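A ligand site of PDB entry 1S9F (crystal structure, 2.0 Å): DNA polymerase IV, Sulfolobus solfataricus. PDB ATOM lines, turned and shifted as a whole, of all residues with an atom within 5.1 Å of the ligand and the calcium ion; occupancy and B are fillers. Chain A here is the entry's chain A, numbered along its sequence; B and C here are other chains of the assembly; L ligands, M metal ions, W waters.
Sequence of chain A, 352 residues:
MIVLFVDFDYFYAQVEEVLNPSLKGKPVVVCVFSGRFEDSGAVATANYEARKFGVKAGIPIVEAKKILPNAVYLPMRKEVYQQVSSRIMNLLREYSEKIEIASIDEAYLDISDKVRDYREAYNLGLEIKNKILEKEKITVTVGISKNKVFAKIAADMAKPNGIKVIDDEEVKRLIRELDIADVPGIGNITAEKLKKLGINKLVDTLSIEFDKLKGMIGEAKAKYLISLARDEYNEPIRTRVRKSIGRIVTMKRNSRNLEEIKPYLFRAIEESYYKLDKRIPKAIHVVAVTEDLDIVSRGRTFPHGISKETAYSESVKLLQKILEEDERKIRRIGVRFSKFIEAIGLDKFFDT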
ATOM      1  N   ASP A   7     -16.358  -2.620 -27.010  1.00  0.00           N
ATOM      2  CA  ASP A   7     -17.036  -3.626 -26.210  1.00  0.00           C
ATOM      3  C   ASP A   7     -18.544  -3.361 -26.241  1.00  0.00           C
ATOM      4  O   ASP A   7     -19.021  -2.403 -25.629  1.00  0.00           O
ATOM      5  CB  ASP A   7     -16.448  -3.548 -24.797  1.00  0.00           C
ATOM      6  CG  ASP A   7     -17.139  -4.444 -23.798  1.00  0.00           C
ATOM      7  OD1 ASP A   7     -16.459  -4.964 -22.892  1.00  0.00           O
ATOM      8  OD2 ASP A   7     -18.360  -4.607 -23.925  1.00  0.00           O
ATOM      9  N   PHE A   8     -19.306  -4.196 -26.954  1.00  0.00           N
ATOM     10  CA  PHE A   8     -20.754  -4.014 -27.080  1.00  0.00           C
ATOM     11  C   PHE A   8     -21.430  -4.080 -25.704  1.00  0.00           C
ATOM     12  O   PHE A   8     -21.110  -4.959 -24.925  1.00  0.00           O
ATOM     13  CB  PHE A   8     -21.362  -5.079 -28.008  1.00  0.00           C
ATOM     14  CG  PHE A   8     -20.613  -5.289 -29.301  1.00  0.00           C
ATOM     15  CD1 PHE A   8     -19.679  -4.342 -29.755  1.00  0.00           C
ATOM     16  CD2 PHE A   8     -20.847  -6.422 -30.072  1.00  0.00           C
ATOM     17  CE1 PHE A   8     -18.987  -4.538 -30.960  1.00  0.00           C
ATOM     18  CE2 PHE A   8     -20.161  -6.626 -31.274  1.00  0.00           C
ATOM     19  CZ  PHE A   8     -19.226  -5.679 -31.728  1.00  0.00           C
ATOM     20  N   ASP A   9     -22.380  -3.187 -25.416  1.00  0.00           N
ATOM     21  CA  ASP A   9     -23.035  -3.190 -24.100  1.00  0.00           C
ATOM     22  C   ASP A   9     -24.071  -4.318 -23.896  1.00  0.00           C
ATOM     23  O   ASP A   9     -24.917  -4.550 -24.767  1.00  0.00           O
ATOM     24  CB  ASP A   9     -23.702  -1.826 -23.852  1.00  0.00           C
ATOM     25  CG  ASP A   9     -22.724  -0.662 -23.977  1.00  0.00           C
ATOM     26  OD1 ASP A   9     -21.575  -0.784 -23.484  1.00  0.00           O
ATOM     27  OD2 ASP A   9     -23.104   0.387 -24.552  1.00  0.00           O
ATOM     28  N   TYR A  10     -24.000  -5.017 -22.752  1.00  0.00           N
ATOM     29  CA  TYR A  10     -24.903  -6.128 -22.415  1.00  0.00           C
ATOM     30  C   TYR A  10     -25.456  -6.768 -23.684  1.00  0.00           C
ATOM     31  O   TYR A  10     -26.677  -6.960 -23.847  1.00  0.00           O
ATOM     32  CB  TYR A  10     -26.048  -5.616 -21.494  1.00  0.00           C
ATOM     33  CG  TYR A  10     -26.948  -4.524 -22.075  1.00  0.00           C
ATOM     34  CD1 TYR A  10     -28.247  -4.813 -22.472  1.00  0.00           C
ATOM     35  CD2 TYR A  10     -26.495  -3.214 -22.214  1.00  0.00           C
ATOM     36  CE1 TYR A  10     -29.080  -3.819 -22.987  1.00  0.00           C
ATOM     37  CE2 TYR A  10     -27.317  -2.205 -22.736  1.00  0.00           C
ATOM     38  CZ  TYR A  10     -28.615  -2.526 -23.115  1.00  0.00           C
ATOM     39  OH  TYR A  10     -29.454  -1.554 -23.630  1.00  0.00           O
ATOM     40  N   PHE A  11     -24.520  -7.132 -24.574  1.00  0.00           N
ATOM     41  CA  PHE A  11     -24.822  -7.612 -25.904  1.00  0.00           C
ATOM     42  C   PHE A  11     -26.025  -8.477 -26.207  1.00  0.00           C
ATOM     43  O   PHE A  11     -26.894  -8.044 -26.965  1.00  0.00           O
ATOM     44  CB  PHE A  11     -23.585  -8.217 -26.555  1.00  0.00           C
ATOM     45  CG  PHE A  11     -23.703  -8.381 -28.054  1.00  0.00           C
ATOM     46  CD1 PHE A  11     -24.178  -7.327 -28.833  1.00  0.00           C
ATOM     47  CD2 PHE A  11     -23.406  -9.590 -28.668  1.00  0.00           C
ATOM     48  CE1 PHE A  11     -24.346  -7.465 -30.204  1.00  0.00           C
ATOM     49  CE2 PHE A  11     -23.570  -9.747 -30.048  1.00  0.00           C
ATOM     50  CZ  PHE A  11     -24.044  -8.679 -30.825  1.00  0.00           C
ATOM     51  N   TYR A  12     -26.088  -9.688 -25.681  1.00  0.00           N
ATOM     52  CA  TYR A  12     -27.235 -10.536 -26.006  1.00  0.00           C
ATOM     53  C   TYR A  12     -28.556  -9.889 -25.633  1.00  0.00           C
ATOM     54  O   TYR A  12     -29.503  -9.872 -26.425  1.00  0.00           O
ATOM     55  CB  TYR A  12     -27.135 -11.893 -25.309  1.00  0.00           C
ATOM     56  CG  TYR A  12     -25.917 -12.716 -25.685  1.00  0.00           C
ATOM     57  CD1 TYR A  12     -25.114 -12.351 -26.765  1.00  0.00           C
ATOM     58  CD2 TYR A  12     -25.594 -13.872 -24.968  1.00  0.00           C
ATOM     59  CE1 TYR A  12     -24.021 -13.119 -27.130  1.00  0.00           C
ATOM     60  CE2 TYR A  12     -24.495 -14.641 -25.327  1.00  0.00           C
ATOM     61  CZ  TYR A  12     -23.708 -14.262 -26.401  1.00  0.00           C
ATOM     62  OH  TYR A  12     -22.605 -15.000 -26.740  1.00  0.00           O
ATOM     63  N   VAL A  43     -27.651 -17.902 -16.345  1.00  0.00           N
ATOM     64  CA  VAL A  43     -27.860 -16.625 -17.013  1.00  0.00           C
ATOM     65  C   VAL A  43     -26.629 -16.319 -17.858  1.00  0.00           C
ATOM     66  O   VAL A  43     -25.503 -16.374 -17.368  1.00  0.00           O
ATOM     67  CB  VAL A  43     -28.061 -15.488 -15.956  1.00  0.00           C
ATOM     68  CG1 VAL A  43     -28.120 -14.133 -16.651  1.00  0.00           C
ATOM     69  CG2 VAL A  43     -29.335 -15.722 -15.135  1.00  0.00           C
ATOM     70  N   ALA A  44     -26.828 -16.018 -19.139  1.00  0.00           N
ATOM     71  CA  ALA A  44     -25.701 -15.678 -20.015  1.00  0.00           C
ATOM     72  C   ALA A  44     -25.371 -14.215 -19.794  1.00  0.00           C
ATOM     73  O   ALA A  44     -24.203 -13.819 -19.695  1.00  0.00           O
ATOM     74  CB  ALA A  44     -26.069 -15.928 -21.491  1.00  0.00           C
ATOM     75  N   THR A  45     -26.416 -13.392 -19.732  1.00  0.00           N
ATOM     76  CA  THR A  45     -26.289 -11.972 -19.463  1.00  0.00           C
ATOM     77  C   THR A  45     -27.658 -11.354 -19.208  1.00  0.00           C
ATOM     78  O   THR A  45     -28.692 -11.946 -19.476  1.00  0.00           O
ATOM     79  CB  THR A  45     -25.607 -11.201 -20.616  1.00  0.00           C
ATOM     80  OG1 THR A  45     -25.412  -9.844 -20.204  1.00  0.00           O
ATOM     81  CG2 THR A  45     -26.463 -11.218 -21.878  1.00  0.00           C
ATOM     82  N   ALA A  46     -27.651 -10.146 -18.665  1.00  0.00           N
ATOM     83  CA  ALA A  46     -28.883  -9.438 -18.363  1.00  0.00           C
ATOM     84  C   ALA A  46     -28.665  -7.955 -18.641  1.00  0.00           C
ATOM     85  O   ALA A  46     -27.530  -7.485 -18.576  1.00  0.00           O
ATOM     86  CB  ALA A  46     -29.240  -9.645 -16.910  1.00  0.00           C
ATOM     87  N   TYR A  48     -28.869  -3.848 -17.888  1.00  0.00           N
ATOM     88  CA  TYR A  48     -28.502  -3.169 -16.655  1.00  0.00           C
ATOM     89  C   TYR A  48     -29.630  -3.000 -15.657  1.00  0.00           C
ATOM     90  O   TYR A  48     -29.379  -2.870 -14.469  1.00  0.00           O
ATOM     91  CB  TYR A  48     -27.811  -1.838 -16.953  1.00  0.00           C
ATOM     92  CG  TYR A  48     -26.358  -2.021 -17.360  1.00  0.00           C
ATOM     93  CD1 TYR A  48     -26.009  -2.460 -18.636  1.00  0.00           C
ATOM     94  CD2 TYR A  48     -25.329  -1.780 -16.439  1.00  0.00           C
ATOM     95  CE1 TYR A  48     -24.666  -2.661 -18.997  1.00  0.00           C
ATOM     96  CE2 TYR A  48     -23.989  -1.985 -16.784  1.00  0.00           C
ATOM     97  CZ  TYR A  48     -23.671  -2.420 -18.070  1.00  0.00           C
ATOM     98  OH  TYR A  48     -22.353  -2.605 -18.403  1.00  0.00           O
ATOM     99  N   ARG A  51     -29.415  -6.024 -13.603  1.00  0.00           N
ATOM    100  CA  ARG A  51     -28.189  -6.061 -12.819  1.00  0.00           C
ATOM    101  C   ARG A  51     -28.305  -5.219 -11.553  1.00  0.00           C
ATOM    102  O   ARG A  51     -27.637  -5.474 -10.565  1.00  0.00           O
ATOM    103  CB  ARG A  51     -26.995  -5.581 -13.653  1.00  0.00           C
ATOM    104  CG  ARG A  51     -26.709  -6.457 -14.868  1.00  0.00           C
ATOM    105  CD  ARG A  51     -25.482  -5.962 -15.645  1.00  0.00           C
ATOM    106  NE  ARG A  51     -25.368  -6.608 -16.943  1.00  0.00           N
ATOM    107  CZ  ARG A  51     -24.292  -6.536 -17.741  1.00  0.00           C
ATOM    108  NH1 ARG A  51     -23.227  -5.840 -17.361  1.00  0.00           N
ATOM    109  NH2 ARG A  51     -24.310  -7.151 -18.915  1.00  0.00           N
ATOM    110  N   ALA A  57     -24.444 -12.489 -15.147  1.00  0.00           N
ATOM    111  CA  ALA A  57     -24.052 -13.672 -15.906  1.00  0.00           C
ATOM    112  C   ALA A  57     -23.461 -14.720 -14.981  1.00  0.00           C
ATOM    113  O   ALA A  57     -22.737 -14.386 -14.048  1.00  0.00           O
ATOM    114  CB  ALA A  57     -23.029 -13.286 -16.967  1.00  0.00           C
ATOM    115  N   GLY A  58     -23.785 -15.976 -15.225  1.00  0.00           N
ATOM    116  CA  GLY A  58     -23.239 -17.049 -14.405  1.00  0.00           C
ATOM    117  C   GLY A  58     -24.128 -17.613 -13.323  1.00  0.00           C
ATOM    118  O   GLY A  58     -23.977 -18.776 -12.967  1.00  0.00           O
ATOM    119  N   ILE A 104     -17.068 -12.618 -29.416  1.00  0.00           N
ATOM    120  CA  ILE A 104     -18.310 -12.206 -30.054  1.00  0.00           C
ATOM    121  C   ILE A 104     -18.660 -10.725 -29.886  1.00  0.00           C
ATOM    122  O   ILE A 104     -19.349 -10.150 -30.741  1.00  0.00           O
ATOM    123  CB  ILE A 104     -19.500 -13.084 -29.559  1.00  0.00           C
ATOM    124  CG1 ILE A 104     -20.716 -12.856 -30.458  1.00  0.00           C
ATOM    125  CG2 ILE A 104     -19.807 -12.780 -28.104  1.00  0.00           C
ATOM    126  CD1 ILE A 104     -21.802 -13.909 -30.284  1.00  0.00           C
ATOM    127  N   ASP A 105     -18.208 -10.087 -28.819  1.00  0.00           N
ATOM    128  CA  ASP A 105     -18.560  -8.685 -28.656  1.00  0.00           C
ATOM    129  C   ASP A 105     -17.428  -7.760 -28.210  1.00  0.00           C
ATOM    130  O   ASP A 105     -17.674  -6.724 -27.579  1.00  0.00           O
ATOM    131  CB  ASP A 105     -19.755  -8.567 -27.705  1.00  0.00           C
ATOM    132  CG  ASP A 105     -19.345  -8.558 -26.264  1.00  0.00           C
ATOM    133  OD1 ASP A 105     -18.420  -9.291 -25.870  1.00  0.00           O
ATOM    134  OD2 ASP A 105     -19.975  -7.786 -25.524  1.00  0.00           O
ATOM    135  N   LYS A 159     -18.057   1.464 -19.264  1.00  0.00           N
ATOM    136  CA  LYS A 159     -19.316   0.847 -19.660  1.00  0.00           C
ATOM    137  C   LYS A 159     -20.435   1.093 -18.650  1.00  0.00           C
ATOM    138  O   LYS A 159     -20.176   1.248 -17.449  1.00  0.00           O
ATOM    139  CB  LYS A 159     -19.141  -0.660 -19.934  1.00  0.00           C
ATOM    140  CG  LYS A 159     -18.699  -1.503 -18.751  1.00  0.00           C
ATOM    141  CD  LYS A 159     -18.600  -3.003 -19.105  1.00  0.00           C
ATOM    142  CE  LYS A 159     -17.609  -3.248 -20.260  1.00  0.00           C
ATOM    143  NZ  LYS A 159     -17.359  -4.706 -20.509  1.00  0.00           N
ATOM    144  P    DG B   5     -24.274 -26.344 -15.489  1.00  0.00           P
ATOM    145  OP1  DG B   5     -25.362 -27.341 -15.341  1.00  0.00           O
ATOM    146  OP2  DG B   5     -22.892 -26.807 -15.789  1.00  0.00           O
ATOM    147  O5'  DG B   5     -24.727 -25.311 -16.611  1.00  0.00           O
ATOM    148  C5'  DG B   5     -26.095 -25.184 -16.973  1.00  0.00           C
ATOM    149  C4'  DG B   5     -26.205 -24.665 -18.384  1.00  0.00           C
ATOM    150  O4'  DG B   5     -25.758 -23.291 -18.415  1.00  0.00           O
ATOM    151  C3'  DG B   5     -25.311 -25.423 -19.351  1.00  0.00           C
ATOM    152  O3'  DG B   5     -25.975 -25.486 -20.614  1.00  0.00           O
ATOM    153  C2'  DG B   5     -24.049 -24.577 -19.412  1.00  0.00           C
ATOM    154  C1'  DG B   5     -24.580 -23.169 -19.200  1.00  0.00           C
ATOM    155  N9   DG B   5     -23.700 -22.251 -18.494  1.00  0.00           N
ATOM    156  C8   DG B   5     -23.173 -22.399 -17.224  1.00  0.00           C
ATOM    157  N7   DG B   5     -22.479 -21.368 -16.832  1.00  0.00           N
ATOM    158  C5   DG B   5     -22.540 -20.485 -17.894  1.00  0.00           C
ATOM    159  C6   DG B   5     -21.990 -19.184 -18.046  1.00  0.00           C
ATOM    160  O6   DG B   5     -21.334 -18.521 -17.245  1.00  0.00           O
ATOM    161  N1   DG B   5     -22.285 -18.646 -19.298  1.00  0.00           N
ATOM    162  C2   DG B   5     -23.010 -19.273 -20.280  1.00  0.00           C
ATOM    163  N2   DG B   5     -23.196 -18.578 -21.412  1.00  0.00           N
ATOM    164  N3   DG B   5     -23.527 -20.491 -20.152  1.00  0.00           N
ATOM    165  C4   DG B   5     -23.262 -21.026 -18.942  1.00  0.00           C
ATOM    166  P    DT B   6     -25.421 -26.465 -21.749  1.00  0.00           P
ATOM    167  OP1  DT B   6     -26.581 -26.743 -22.638  1.00  0.00           O
ATOM    168  OP2  DT B   6     -24.684 -27.588 -21.117  1.00  0.00           O
ATOM    169  O5'  DT B   6     -24.420 -25.539 -22.560  1.00  0.00           O
ATOM    170  C5'  DT B   6     -24.943 -24.452 -23.312  1.00  0.00           C
ATOM    171  C4'  DT B   6     -23.841 -23.640 -23.953  1.00  0.00           C
ATOM    172  O4'  DT B   6     -23.174 -22.773 -22.993  1.00  0.00           O
ATOM    173  C3'  DT B   6     -22.746 -24.409 -24.678  1.00  0.00           C
ATOM    174  O3'  DT B   6     -22.618 -23.807 -25.959  1.00  0.00           O
ATOM    175  C2'  DT B   6     -21.507 -24.146 -23.843  1.00  0.00           C
ATOM    176  C1'  DT B   6     -21.802 -22.754 -23.310  1.00  0.00           C
ATOM    177  N1   DT B   6     -21.064 -22.313 -22.105  1.00  0.00           N
ATOM    178  C2   DT B   6     -20.541 -21.039 -22.124  1.00  0.00           C
ATOM    179  O2   DT B   6     -20.612 -20.300 -23.086  1.00  0.00           O
ATOM    180  N3   DT B   6     -19.916 -20.655 -20.966  1.00  0.00           N
ATOM    181  C4   DT B   6     -19.754 -21.408 -19.827  1.00  0.00           C
ATOM    182  O4   DT B   6     -19.190 -20.916 -18.850  1.00  0.00           O
ATOM    183  C5   DT B   6     -20.300 -22.746 -19.873  1.00  0.00           C
ATOM    184  C7   DT B   6     -20.145 -23.645 -18.694  1.00  0.00           C
ATOM    185  C6   DT B   6     -20.926 -23.129 -21.002  1.00  0.00           C
ATOM    186  P    DA C  13     -13.886 -10.316 -20.652  1.00  0.00           P
ATOM    187  OP1  DA C  13     -13.716  -8.887 -21.009  1.00  0.00           O
ATOM    188  OP2  DA C  13     -14.360 -10.678 -19.295  1.00  0.00           O
ATOM    189  O5'  DA C  13     -14.836 -11.006 -21.727  1.00  0.00           O
ATOM    190  C5'  DA C  13     -14.348 -11.308 -23.031  1.00  0.00           C
ATOM    191  C4'  DA C  13     -15.310 -12.199 -23.778  1.00  0.00           C
ATOM    192  O4'  DA C  13     -15.387 -13.506 -23.136  1.00  0.00           O
ATOM    193  C3'  DA C  13     -16.750 -11.702 -23.886  1.00  0.00           C
ATOM    194  O3'  DA C  13     -17.352 -12.257 -25.069  1.00  0.00           O
ATOM    195  C2'  DA C  13     -17.453 -12.482 -22.787  1.00  0.00           C
ATOM    196  C1'  DA C  13     -16.757 -13.820 -22.928  1.00  0.00           C
ATOM    197  N9   DA C  13     -16.858 -14.678 -21.743  1.00  0.00           N
ATOM    198  C8   DA C  13     -16.393 -14.441 -20.466  1.00  0.00           C
ATOM    199  N7   DA C  13     -16.695 -15.396 -19.623  1.00  0.00           N
ATOM    200  C5   DA C  13     -17.391 -16.312 -20.382  1.00  0.00           C
ATOM    201  C6   DA C  13     -18.006 -17.531 -20.058  1.00  0.00           C
ATOM    202  N6   DA C  13     -18.018 -18.055 -18.829  1.00  0.00           N
ATOM    203  N1   DA C  13     -18.628 -18.211 -21.055  1.00  0.00           N
ATOM    204  C2   DA C  13     -18.628 -17.678 -22.285  1.00  0.00           C
ATOM    205  N3   DA C  13     -18.094 -16.536 -22.707  1.00  0.00           N
ATOM    206  C4   DA C  13     -17.493 -15.887 -21.697  1.00  0.00           C
HETATM  207  C1  LIG L   1     -20.490 -15.103 -18.994  1.00  0.00           C
HETATM  208  P1  LIG L   1     -20.458  -6.915 -20.031  1.00  0.00           P
HETATM  209  P2  LIG L   1     -22.038  -8.512 -21.857  1.00  0.00           P
HETATM  210  C2  LIG L   1     -21.507 -15.411 -21.188  1.00  0.00           C
HETATM  211  C3  LIG L   1     -20.143 -13.789 -19.328  1.00  0.00           C
HETATM  212  O1  LIG L   1     -22.116 -16.129 -21.980  1.00  0.00           O
HETATM  213  O2  LIG L   1     -21.839  -6.182 -19.676  1.00  0.00           O
HETATM  214  O3  LIG L   1     -19.765  -6.066 -21.016  1.00  0.00           O
HETATM  215  O4  LIG L   1     -19.761  -7.230 -18.773  1.00  0.00           O
HETATM  216  O5  LIG L   1     -20.920  -8.334 -20.696  1.00  0.00           O
HETATM  217  O6  LIG L   1     -21.901  -7.489 -22.905  1.00  0.00           O
HETATM  218  O7  LIG L   1     -23.360  -8.642 -21.205  1.00  0.00           O
HETATM  219  O8  LIG L   1     -21.625  -9.949 -22.447  1.00  0.00           O
HETATM  220  C4  LIG L   1     -21.273 -10.143 -23.816  1.00  0.00           C
HETATM  221  C5  LIG L   1     -21.404 -11.638 -24.142  1.00  0.00           C
HETATM  222  O9  LIG L   1     -20.562 -12.452 -23.288  1.00  0.00           O
HETATM  223  C6  LIG L   1     -22.645 -12.044 -23.842  1.00  0.00           C
HETATM  224  C7  LIG L   1     -22.632 -13.152 -23.136  1.00  0.00           C
HETATM  225  C8  LIG L   1     -21.398 -13.588 -22.925  1.00  0.00           C
HETATM  226  N1  LIG L   1     -21.145 -14.088 -21.536  1.00  0.00           N
HETATM  227  C9  LIG L   1     -20.464 -13.277 -20.591  1.00  0.00           C
HETATM  228  N2  LIG L   1     -20.168 -15.595 -17.800  1.00  0.00           N
HETATM  229  N3  LIG L   1     -21.167 -15.906 -19.913  1.00  0.00           N
HETATM  230 CA    CA M   1     -19.898  -6.432 -23.453  1.00  0.00          CA
HETATM  231  O   HOH W   1     -22.992 -10.487 -19.215  1.00  0.00           O
HETATM  232  O   HOH W   2     -20.839  -9.819 -17.957  1.00  0.00           O
HETATM  233  O   HOH W   3     -18.916 -13.875 -15.960  1.00  0.00           O
HETATM  234  O   HOH W   4     -22.153  -3.861 -20.963  1.00  0.00           O
HETATM  235  O   HOH W   5     -21.836 -16.669 -24.857  1.00  0.00           O
HETATM  236  O   HOH W   6     -19.423  -6.120 -16.539  1.00  0.00           O
HETATM  237  O   HOH W   7     -17.812  -8.073 -23.030  1.00  0.00           O
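An oxygen (O7) of the ligand is in hydrogen-bond range of the side-chain hydroxyl (OG1) of Thr 45 (2.6 Å).
O2 of the ligand is in salt-bridge range of NH1 of Arg 51.
O6 of DG 5 of chain B lies within hydrogen-bond range of N2 of the ligand.
An oxygen (O4) of the ligand lies within salt-bridge range of the side-chain amino group (NZ) of Lys 159.
An oxygen (O6) of the ligand sits close to the backbone NH (N) of Phe 11 (3.1 Å).
A nitrogen (N2) of the ligand sits at hydrogen-bond distance from N6 of DA 13 of chain C.
The backbone NH (N) of Tyr 10 sits close to an oxygen (O6) of the ligand, at 3.2 Å.
OD1 of Asp 7 is in salt-bridge range of NZ of Lys 159 (2.6 Å).
The guanidinium group (NH2) of Arg 51 lies within hydrogen-bond range of the side-chain hydroxyl (OG1) of Thr 45 (3.2 Å).
The backbone carbonyl oxygen (O) of Ala 46 is in hydrogen-bond range of the guanidinium group (NE) of Arg 51.
C of Asp 9 touches O6 of the ligand (3.97 Å).
Tyr 12 touches the ligand.
O of Ala 44 touches C2 of the ligand (3.5 Å).
Tyr 48 touches the ligand (OH to O2, 3.8 Å).
CB of Ala 57 touches C1 of the ligand, 3.7 Å away.
Hydrophobic or aromatic side chains that line the ligand: Tyr 12, Ala 44 and Ala 57.
15 residues have an atom within 4 Å of the ligand: Asp 7, Phe 8, Asp 9, Tyr 10, Phe 11, Tyr 12, Ala 44, Thr 45, Tyr 48, Arg 51, Ala 57, Asp 105, Lys 159, DG 5 of chain B and DA 13 of chain C.
Along chain A the residues within 4 Å of the ligand span positions 7 to 159.
The nearest printed residue that does not touch the ligand is Ile 104 (4.4 Å).
The nearest printed residue that does not touch the calcium ion is Lys 159 (4.3 Å).
The calcium ion is bound by O6 of the ligand (2.3 Å).
The calcium ion is bound by O of Phe 8, 2.4 Å away.
The calcium ion is bound by the side-chain carboxylate (OD2) of Asp 7, 2.4 Å away.
The calcium ion is bound by an oxygen (O3) of the ligand, 2.5 Å away.
The calcium ion is bound by the side-chain carboxylate (OD2) of Asp 105 (2.5 Å).
Water W7 binds the calcium ion.
The calcium ion has six donor atoms within binding distance.
Water W7 lies within hydrogen-bond range of OD1 of Asp 105 and OD1 of Asp 7.
Water W4 lies within hydrogen-bond range of O2 of the ligand (2.7 Å), N of Tyr 10 (2.8 Å) and OH of Tyr 48 (2.9 Å).
Water W1 bridges the side-chain hydroxyl (OG1) of Thr 45 and an oxygen (O7) of the ligand.
Water W5 lies within hydrogen-bond range of the side-chain hydroxyl (OH) of Tyr 12 (2.6 Å) and an oxygen (O1) of the ligand (2.9 Å).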
